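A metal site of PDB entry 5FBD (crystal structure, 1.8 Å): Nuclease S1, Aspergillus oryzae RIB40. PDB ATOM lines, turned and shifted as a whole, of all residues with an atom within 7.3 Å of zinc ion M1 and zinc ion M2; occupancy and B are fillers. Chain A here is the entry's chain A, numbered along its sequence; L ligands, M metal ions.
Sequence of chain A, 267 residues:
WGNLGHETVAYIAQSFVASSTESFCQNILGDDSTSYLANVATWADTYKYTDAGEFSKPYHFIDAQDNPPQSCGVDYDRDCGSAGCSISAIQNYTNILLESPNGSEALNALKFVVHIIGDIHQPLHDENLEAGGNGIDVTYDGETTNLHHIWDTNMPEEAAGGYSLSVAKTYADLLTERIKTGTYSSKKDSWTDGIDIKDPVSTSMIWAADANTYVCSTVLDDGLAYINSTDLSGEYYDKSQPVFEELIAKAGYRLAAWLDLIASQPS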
ATOM      1  N   TRP A   1       5.502 -15.628 -27.287  1.00  0.00           N
ATOM      2  CA  TRP A   1       6.750 -14.906 -27.132  1.00  0.00           C
ATOM      3  C   TRP A   1       6.862 -13.998 -28.320  1.00  0.00           C
ATOM      4  O   TRP A   1       6.255 -14.257 -29.347  1.00  0.00           O
ATOM      5  CB  TRP A   1       7.971 -15.831 -27.094  1.00  0.00           C
ATOM      6  CG  TRP A   1       7.874 -16.896 -26.051  1.00  0.00           C
ATOM      7  CD1 TRP A   1       7.555 -18.192 -26.259  1.00  0.00           C
ATOM      8  CD2 TRP A   1       7.993 -16.719 -24.634  1.00  0.00           C
ATOM      9  NE1 TRP A   1       7.550 -18.869 -25.061  1.00  0.00           N
ATOM     10  CE2 TRP A   1       7.828 -17.993 -24.049  1.00  0.00           C
ATOM     11  CE3 TRP A   1       8.288 -15.617 -23.809  1.00  0.00           C
ATOM     12  CZ2 TRP A   1       7.843 -18.197 -22.672  1.00  0.00           C
ATOM     13  CZ3 TRP A   1       8.354 -15.807 -22.460  1.00  0.00           C
ATOM     14  CH2 TRP A   1       8.154 -17.125 -21.876  1.00  0.00           C
ATOM     15  N   GLY A   2       7.708 -13.002 -28.195  1.00  0.00           N
ATOM     16  CA  GLY A   2       8.185 -12.218 -29.335  1.00  0.00           C
ATOM     17  C   GLY A   2       9.202 -13.052 -30.069  1.00  0.00           C
ATOM     18  O   GLY A   2       9.474 -14.231 -29.736  1.00  0.00           O
ATOM     19  N   ASN A   3       9.755 -12.434 -31.090  1.00  0.00           N
ATOM     20  CA  ASN A   3      10.608 -13.139 -32.017  1.00  0.00           C
ATOM     21  C   ASN A   3      11.778 -13.771 -31.307  1.00  0.00           C
ATOM     22  O   ASN A   3      12.096 -14.920 -31.571  1.00  0.00           O
ATOM     23  CB  ASN A   3      11.096 -12.228 -33.145  1.00  0.00           C
ATOM     24  CG  ASN A   3      10.000 -11.816 -34.101  1.00  0.00           C
ATOM     25  OD1 ASN A   3       8.911 -12.387 -34.164  1.00  0.00           O
ATOM     26  ND2 ASN A   3      10.291 -10.788 -34.879  1.00  0.00           N
ATOM     27  N   GLY A   5      12.161 -14.821 -28.196  1.00  0.00           N
ATOM     28  CA  GLY A   5      11.787 -16.018 -27.470  1.00  0.00           C
ATOM     29  C   GLY A   5      11.531 -17.207 -28.350  1.00  0.00           C
ATOM     30  O   GLY A   5      11.958 -18.320 -28.012  1.00  0.00           O
ATOM     31  N   HIS A   6      10.861 -17.012 -29.484  1.00  0.00           N
ATOM     32  CA  HIS A   6      10.593 -18.126 -30.392  1.00  0.00           C
ATOM     33  C   HIS A   6      11.869 -18.709 -30.977  1.00  0.00           C
ATOM     34  O   HIS A   6      11.977 -19.944 -31.164  1.00  0.00           O
ATOM     35  CB  HIS A   6       9.661 -17.698 -31.523  1.00  0.00           C
ATOM     36  CG  HIS A   6       8.244 -17.600 -31.066  1.00  0.00           C
ATOM     37  ND1 HIS A   6       7.510 -18.715 -30.737  1.00  0.00           N
ATOM     38  CD2 HIS A   6       7.455 -16.524 -30.787  1.00  0.00           C
ATOM     39  CE1 HIS A   6       6.316 -18.343 -30.274  1.00  0.00           C
ATOM     40  NE2 HIS A   6       6.281 -17.018 -30.256  1.00  0.00           N
ATOM     41  N   ALA A  41      10.699 -20.008 -36.972  1.00  0.00           N
ATOM     42  CA  ALA A  41      10.007 -19.979 -35.703  1.00  0.00           C
ATOM     43  C   ALA A  41       9.073 -18.810 -35.511  1.00  0.00           C
ATOM     44  O   ALA A  41       8.255 -18.873 -34.599  1.00  0.00           O
ATOM     45  CB  ALA A  41      10.994 -20.023 -34.547  1.00  0.00           C
ATOM     46  N   THR A  42       9.209 -17.754 -36.329  1.00  0.00           N
ATOM     47  CA  THR A  42       8.404 -16.515 -36.183  1.00  0.00           C
ATOM     48  C   THR A  42       7.322 -16.442 -37.275  1.00  0.00           C
ATOM     49  O   THR A  42       6.428 -15.631 -37.172  1.00  0.00           O
ATOM     50  CB  THR A  42       9.271 -15.232 -36.251  1.00  0.00           C
ATOM     51  OG1 THR A  42       9.855 -15.145 -37.549  1.00  0.00           O
ATOM     52  CG2 THR A  42      10.352 -15.259 -35.199  1.00  0.00           C
ATOM     53  N   ALA A  44       4.582 -17.912 -38.162  1.00  0.00           N
ATOM     54  CA  ALA A  44       3.151 -17.982 -37.812  1.00  0.00           C
ATOM     55  C   ALA A  44       2.617 -16.644 -37.310  1.00  0.00           C
ATOM     56  O   ALA A  44       1.448 -16.323 -37.561  1.00  0.00           O
ATOM     57  CB  ALA A  44       2.863 -19.109 -36.816  1.00  0.00           C
ATOM     58  N   ASP A  45       3.498 -15.804 -36.738  1.00  0.00           N
ATOM     59  CA  ASP A  45       3.065 -14.522 -36.155  1.00  0.00           C
ATOM     60  C   ASP A  45       2.840 -13.441 -37.169  1.00  0.00           C
ATOM     61  O   ASP A  45       2.057 -12.569 -36.938  1.00  0.00           O
ATOM     62  CB  ASP A  45       4.025 -14.030 -35.062  1.00  0.00           C
ATOM     63  CG  ASP A  45       3.694 -14.600 -33.700  1.00  0.00           C
ATOM     64  OD1 ASP A  45       2.595 -15.240 -33.516  1.00  0.00           O
ATOM     65  OD2 ASP A  45       4.543 -14.434 -32.806  1.00  0.00           O
ATOM     66  N   LYS A  48      -0.487 -14.984 -39.647  1.00  0.00           N
ATOM     67  CA  LYS A  48      -1.827 -14.795 -39.135  1.00  0.00           C
ATOM     68  C   LYS A  48      -2.498 -13.474 -39.429  1.00  0.00           C
ATOM     69  O   LYS A  48      -3.722 -13.347 -39.215  1.00  0.00           O
ATOM     70  CB  LYS A  48      -1.892 -15.037 -37.624  1.00  0.00           C
ATOM     71  CG  LYS A  48      -1.186 -13.969 -36.771  1.00  0.00           C
ATOM     72  CD  LYS A  48      -0.976 -14.487 -35.375  1.00  0.00           C
ATOM     73  CE  LYS A  48      -0.384 -13.466 -34.411  1.00  0.00           C
ATOM     74  NZ  LYS A  48      -0.027 -14.048 -33.084  1.00  0.00           N
ATOM     75  N   LYS A  57      -5.012 -17.240 -36.520  1.00  0.00           N
ATOM     76  CA  LYS A  57      -4.793 -16.375 -35.352  1.00  0.00           C
ATOM     77  C   LYS A  57      -5.129 -17.067 -34.023  1.00  0.00           C
ATOM     78  O   LYS A  57      -4.389 -16.923 -33.068  1.00  0.00           O
ATOM     79  CB  LYS A  57      -5.535 -15.053 -35.528  1.00  0.00           C
ATOM     80  CG  LYS A  57      -5.160 -14.010 -34.507  1.00  0.00           C
ATOM     81  CD  LYS A  57      -5.840 -12.681 -34.827  1.00  0.00           C
ATOM     82  CE  LYS A  57      -5.710 -12.365 -36.306  1.00  0.00           C
ATOM     83  NZ  LYS A  57      -6.297 -11.031 -36.570  1.00  0.00           N
ATOM     84  N   TYR A  59      -4.902 -20.083 -33.089  1.00  0.00           N
ATOM     85  CA  TYR A  59      -3.993 -21.160 -32.773  1.00  0.00           C
ATOM     86  C   TYR A  59      -2.832 -20.802 -31.874  1.00  0.00           C
ATOM     87  O   TYR A  59      -2.063 -21.692 -31.547  1.00  0.00           O
ATOM     88  CB  TYR A  59      -3.419 -21.795 -34.034  1.00  0.00           C
ATOM     89  CG  TYR A  59      -4.446 -22.315 -35.058  1.00  0.00           C
ATOM     90  CD1 TYR A  59      -5.795 -22.406 -34.781  1.00  0.00           C
ATOM     91  CD2 TYR A  59      -4.022 -22.663 -36.322  1.00  0.00           C
ATOM     92  CE1 TYR A  59      -6.699 -22.836 -35.719  1.00  0.00           C
ATOM     93  CE2 TYR A  59      -4.902 -23.140 -37.274  1.00  0.00           C
ATOM     94  CZ  TYR A  59      -6.236 -23.235 -36.965  1.00  0.00           C
ATOM     95  OH  TYR A  59      -7.139 -23.721 -37.920  1.00  0.00           O
ATOM     96  N   HIS A  60      -2.688 -19.567 -31.470  1.00  0.00           N
ATOM     97  CA  HIS A  60      -1.516 -19.142 -30.695  1.00  0.00           C
ATOM     98  C   HIS A  60      -1.680 -19.276 -29.189  1.00  0.00           C
ATOM     99  O   HIS A  60      -0.705 -19.064 -28.433  1.00  0.00           O
ATOM    100  CB  HIS A  60      -1.072 -17.762 -31.117  1.00  0.00           C
ATOM    101  CG  HIS A  60      -0.563 -17.712 -32.518  1.00  0.00           C
ATOM    102  ND1 HIS A  60       0.763 -17.437 -32.825  1.00  0.00           N
ATOM    103  CD2 HIS A  60      -1.175 -17.992 -33.696  1.00  0.00           C
ATOM    104  CE1 HIS A  60       0.906 -17.437 -34.131  1.00  0.00           C
ATOM    105  NE2 HIS A  60      -0.234 -17.855 -34.667  1.00  0.00           N
ATOM    106  N   PHE A  61      -2.903 -19.528 -28.739  1.00  0.00           N
ATOM    107  CA  PHE A  61      -3.174 -19.508 -27.314  1.00  0.00           C
ATOM    108  C   PHE A  61      -4.368 -20.394 -26.977  1.00  0.00           C
ATOM    109  O   PHE A  61      -5.064 -20.930 -27.870  1.00  0.00           O
ATOM    110  CB  PHE A  61      -3.445 -18.064 -26.846  1.00  0.00           C
ATOM    111  CG  PHE A  61      -4.486 -17.353 -27.684  1.00  0.00           C
ATOM    112  CD1 PHE A  61      -5.819 -17.501 -27.422  1.00  0.00           C
ATOM    113  CD2 PHE A  61      -4.104 -16.584 -28.749  1.00  0.00           C
ATOM    114  CE1 PHE A  61      -6.785 -16.834 -28.191  1.00  0.00           C
ATOM    115  CE2 PHE A  61      -5.061 -15.951 -29.554  1.00  0.00           C
ATOM    116  CZ  PHE A  61      -6.399 -16.079 -29.254  1.00  0.00           C
ATOM    117  N   HIS A 115       6.548 -23.012 -33.668  1.00  0.00           N
ATOM    118  CA  HIS A 115       6.091 -21.746 -33.081  1.00  0.00           C
ATOM    119  C   HIS A 115       5.183 -21.987 -31.858  1.00  0.00           C
ATOM    120  O   HIS A 115       5.357 -21.338 -30.832  1.00  0.00           O
ATOM    121  CB  HIS A 115       5.246 -20.971 -34.107  1.00  0.00           C
ATOM    122  CG  HIS A 115       4.857 -19.614 -33.625  1.00  0.00           C
ATOM    123  ND1 HIS A 115       5.714 -18.523 -33.685  1.00  0.00           N
ATOM    124  CD2 HIS A 115       3.760 -19.187 -33.000  1.00  0.00           C
ATOM    125  CE1 HIS A 115       5.105 -17.479 -33.174  1.00  0.00           C
ATOM    126  NE2 HIS A 115       3.921 -17.863 -32.738  1.00  0.00           N
ATOM    127  N   ILE A 116       4.188 -22.842 -32.046  1.00  0.00           N
ATOM    128  CA  ILE A 116       3.114 -23.017 -31.057  1.00  0.00           C
ATOM    129  C   ILE A 116       3.598 -23.728 -29.819  1.00  0.00           C
ATOM    130  O   ILE A 116       3.184 -23.339 -28.740  1.00  0.00           O
ATOM    131  CB  ILE A 116       1.869 -23.650 -31.644  1.00  0.00           C
ATOM    132  CG1 ILE A 116       1.316 -22.666 -32.700  1.00  0.00           C
ATOM    133  CG2 ILE A 116       0.830 -23.927 -30.574  1.00  0.00           C
ATOM    134  CD1 ILE A 116       0.264 -23.177 -33.611  1.00  0.00           C
ATOM    135  N   GLY A 118       6.452 -23.227 -28.507  1.00  0.00           N
ATOM    136  CA  GLY A 118       6.921 -22.082 -27.759  1.00  0.00           C
ATOM    137  C   GLY A 118       5.808 -21.240 -27.130  1.00  0.00           C
ATOM    138  O   GLY A 118       5.931 -20.863 -25.935  1.00  0.00           O
ATOM    139  N   ASP A 119       4.745 -20.878 -27.910  1.00  0.00           N
ATOM    140  CA  ASP A 119       3.657 -20.018 -27.361  1.00  0.00           C
ATOM    141  C   ASP A 119       2.976 -20.645 -26.160  1.00  0.00           C
ATOM    142  O   ASP A 119       2.642 -19.962 -25.230  1.00  0.00           O
ATOM    143  CB  ASP A 119       2.590 -19.683 -28.427  1.00  0.00           C
ATOM    144  CG  ASP A 119       2.899 -18.395 -29.196  1.00  0.00           C
ATOM    145  OD1 ASP A 119       3.754 -17.642 -28.720  1.00  0.00           O
ATOM    146  OD2 ASP A 119       2.291 -18.142 -30.257  1.00  0.00           O
ATOM    147  N   ILE A 120       2.779 -21.973 -26.186  1.00  0.00           N
ATOM    148  CA  ILE A 120       2.155 -22.699 -25.064  1.00  0.00           C
ATOM    149  C   ILE A 120       2.913 -22.467 -23.763  1.00  0.00           C
ATOM    150  O   ILE A 120       2.316 -22.385 -22.697  1.00  0.00           O
ATOM    151  CB  ILE A 120       2.021 -24.163 -25.400  1.00  0.00           C
ATOM    152  CG1 ILE A 120       0.952 -24.346 -26.503  1.00  0.00           C
ATOM    153  CG2 ILE A 120       1.686 -25.009 -24.172  1.00  0.00           C
ATOM    154  CD1 ILE A 120       0.908 -25.770 -26.982  1.00  0.00           C
ATOM    155  N   GLN A 122       4.412 -19.702 -22.806  1.00  0.00           N
ATOM    156  CA  GLN A 122       4.297 -18.340 -22.345  1.00  0.00           C
ATOM    157  C   GLN A 122       2.981 -18.323 -21.505  1.00  0.00           C
ATOM    158  O   GLN A 122       1.919 -18.531 -22.051  1.00  0.00           O
ATOM    159  CB  GLN A 122       4.254 -17.340 -23.515  1.00  0.00           C
ATOM    160  CG  GLN A 122       4.705 -15.926 -23.170  1.00  0.00           C
ATOM    161  CD  GLN A 122       3.716 -15.118 -22.329  1.00  0.00           C
ATOM    162  OE1 GLN A 122       3.324 -15.522 -21.206  1.00  0.00           O
ATOM    163  NE2 GLN A 122       3.312 -13.947 -22.829  1.00  0.00           N
ATOM    164  N   HIS A 125      -0.328 -16.921 -22.670  1.00  0.00           N
ATOM    165  CA  HIS A 125      -0.965 -17.630 -23.804  1.00  0.00           C
ATOM    166  C   HIS A 125      -1.831 -18.803 -23.354  1.00  0.00           C
ATOM    167  O   HIS A 125      -2.385 -19.530 -24.198  1.00  0.00           O
ATOM    168  CB  HIS A 125       0.130 -18.149 -24.743  1.00  0.00           C
ATOM    169  CG  HIS A 125       0.663 -17.105 -25.685  1.00  0.00           C
ATOM    170  ND1 HIS A 125       0.431 -17.153 -27.040  1.00  0.00           N
ATOM    171  CD2 HIS A 125       1.383 -15.980 -25.470  1.00  0.00           C
ATOM    172  CE1 HIS A 125       0.926 -16.085 -27.620  1.00  0.00           C
ATOM    173  NE2 HIS A 125       1.556 -15.376 -26.692  1.00  0.00           N
ATOM    174  N   HIS A 148       0.882  -8.577 -21.381  1.00  0.00           N
ATOM    175  CA  HIS A 148       1.240  -9.561 -22.385  1.00  0.00           C
ATOM    176  C   HIS A 148       2.569  -9.226 -23.110  1.00  0.00           C
ATOM    177  O   HIS A 148       3.465 -10.101 -23.241  1.00  0.00           O
ATOM    178  CB  HIS A 148       0.100  -9.733 -23.360  1.00  0.00           C
ATOM    179  CG  HIS A 148       0.282 -10.924 -24.258  1.00  0.00           C
ATOM    180  ND1 HIS A 148      -0.346 -12.131 -24.031  1.00  0.00           N
ATOM    181  CD2 HIS A 148       1.082 -11.117 -25.332  1.00  0.00           C
ATOM    182  CE1 HIS A 148       0.000 -12.980 -24.976  1.00  0.00           C
ATOM    183  NE2 HIS A 148       0.871 -12.397 -25.766  1.00  0.00           N
ATOM    184  N   ASP A 152       5.978 -11.400 -23.443  1.00  0.00           N
ATOM    185  CA  ASP A 152       6.407 -11.852 -24.748  1.00  0.00           C
ATOM    186  C   ASP A 152       7.744 -11.303 -25.125  1.00  0.00           C
ATOM    187  O   ASP A 152       8.594 -12.012 -25.711  1.00  0.00           O
ATOM    188  CB  ASP A 152       5.385 -11.416 -25.854  1.00  0.00           C
ATOM    189  CG  ASP A 152       4.352 -12.493 -26.188  1.00  0.00           C
ATOM    190  OD1 ASP A 152       4.222 -13.550 -25.527  1.00  0.00           O
ATOM    191  OD2 ASP A 152       3.689 -12.224 -27.170  1.00  0.00           O
HETATM  192  P1  LIG L   1       2.286 -14.106 -30.109  1.00  0.00           P
HETATM  193  O1  LIG L   1       3.555 -14.489 -29.405  1.00  0.00           O
HETATM  194  O2  LIG L   1       1.538 -15.216 -30.806  1.00  0.00           O
HETATM  195  O3  LIG L   1       1.504 -13.416 -29.016  1.00  0.00           O
HETATM  196  O4  LIG L   1       2.570 -13.038 -31.176  1.00  0.00           O
HETATM  197  N1  LG2 L   2      -3.016 -13.306 -27.562  1.00  0.00           N
HETATM  198  C1  LG2 L   2      -3.134 -14.234 -26.525  1.00  0.00           C
HETATM  199  N2  LG2 L   2      -4.347 -14.432 -25.962  1.00  0.00           N
HETATM  200  C2  LG2 L   2      -5.415 -13.725 -26.404  1.00  0.00           C
HETATM  201  C3  LG2 L   2      -5.306 -12.780 -27.456  1.00  0.00           C
HETATM  202  C4  LG2 L   2      -4.102 -12.602 -27.983  1.00  0.00           C
HETATM  203  O1  LG2 L   2      -2.112 -14.857 -26.158  1.00  0.00           O
HETATM  204  N3  LG2 L   2      -6.580 -13.945 -25.848  1.00  0.00           N
HETATM  205  C5  LG2 L   2      -1.704 -13.059 -28.144  1.00  0.00           C
HETATM  206  C6  LG2 L   2      -1.715 -13.258 -29.659  1.00  0.00           C
HETATM  207  C7  LG2 L   2      -1.539 -11.857 -30.233  1.00  0.00           C
HETATM  208  C8  LG2 L   2      -0.925 -11.057 -29.094  1.00  0.00           C
HETATM  209  O2  LG2 L   2      -1.383 -11.692 -27.885  1.00  0.00           O
HETATM  210  O3  LG2 L   2      -0.557 -11.944 -31.260  1.00  0.00           O
HETATM  211  C9  LG2 L   2      -1.287  -9.584 -29.067  1.00  0.00           C
HETATM  212  O4  LG2 L   2      -2.675  -9.375 -29.418  1.00  0.00           O
HETATM  213 ZN    ZN M   1       4.858 -15.931 -29.215  1.00  0.00          ZN
HETATM  214 ZN    ZN M   2       2.325 -16.770 -31.785  1.00  0.00          ZN
HETATM  215 ZN    ZN M   3       2.021 -13.418 -27.175  1.00  0.00          ZN
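NZ of Lys 48 lies within hydrogen-bond range of O3 of LG2 L2 (2.8 Å).
An oxygen (O2) of LG2 L2 lies close to a ring nitrogen (NE2) of His 148 (3.2 Å).
Four residues have an atom within 4 Å of zinc ion M1: Trp 1, His 6, Asp 45 and Asp 119.
The nearest printed residue that does not touch zinc ion M1 is His 115 (4.1 Å).
Zinc ion M1 is bound by O1 of LIG L1.
The backbone nitrogen (N) of Trp 1 is bound to zinc ion M1 (2.1 Å).
Zinc ion M1 is bound by NE2 of His 6 (2.1 Å).
The side-chain carboxylate (OD1) of Asp 119 binds zinc ion M1, 2.1 Å away.
O of Trp 1 is bound to zinc ion M1, at 2.2 Å.
Zinc ion M1 has five donor atoms within binding distance.
A ring nitrogen (ND1) of His 125 lies within hydrogen-bond range of the backbone carbonyl oxygen (O) of His 60 (2.6 Å).
The backbone carbonyl oxygen of His 115 lies close to a ring nitrogen (ND1) of His 6.
NZ of Lys 48 sits close to ND1 of His 60 (3.5 Å).
The backbone NH (N) of Trp 1 lies close to the side-chain carboxylate (OD1) of Asp 152, at 3.0 Å.
ND1 of His 115 sits at hydrogen-bond distance from O of Ala 41 (2.7 Å).
The side-chain amino group (NZ) of Lys 48 lies close to the side-chain carboxylate (OD1) of Asp 45.
O of Gly 118 lies within hydrogen-bond range of NE1 of Trp 1 (2.7 Å).
Merely in contact with zinc ion M2: Lys 48 (3.8 Å).
Five residues have an atom within 4 Å of zinc ion M2: Asp 45, Lys 48, His 60, His 115 and Asp 119.
Zinc ion M2 is bound by ND1 of His 60, 2.0 Å away.
O2 of LIG L1 is bound to zinc ion M2 (2.0 Å).
Zinc ion M2 is bound by OD2 of Asp 119, 2.1 Å away.
Zinc ion M2 is bound by NE2 of His 115 (2.2 Å).
Zinc ion M2 is bound by OD1 of Asp 45 (2.3 Å).
Zinc ion M2 has five donor atoms within binding distance.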
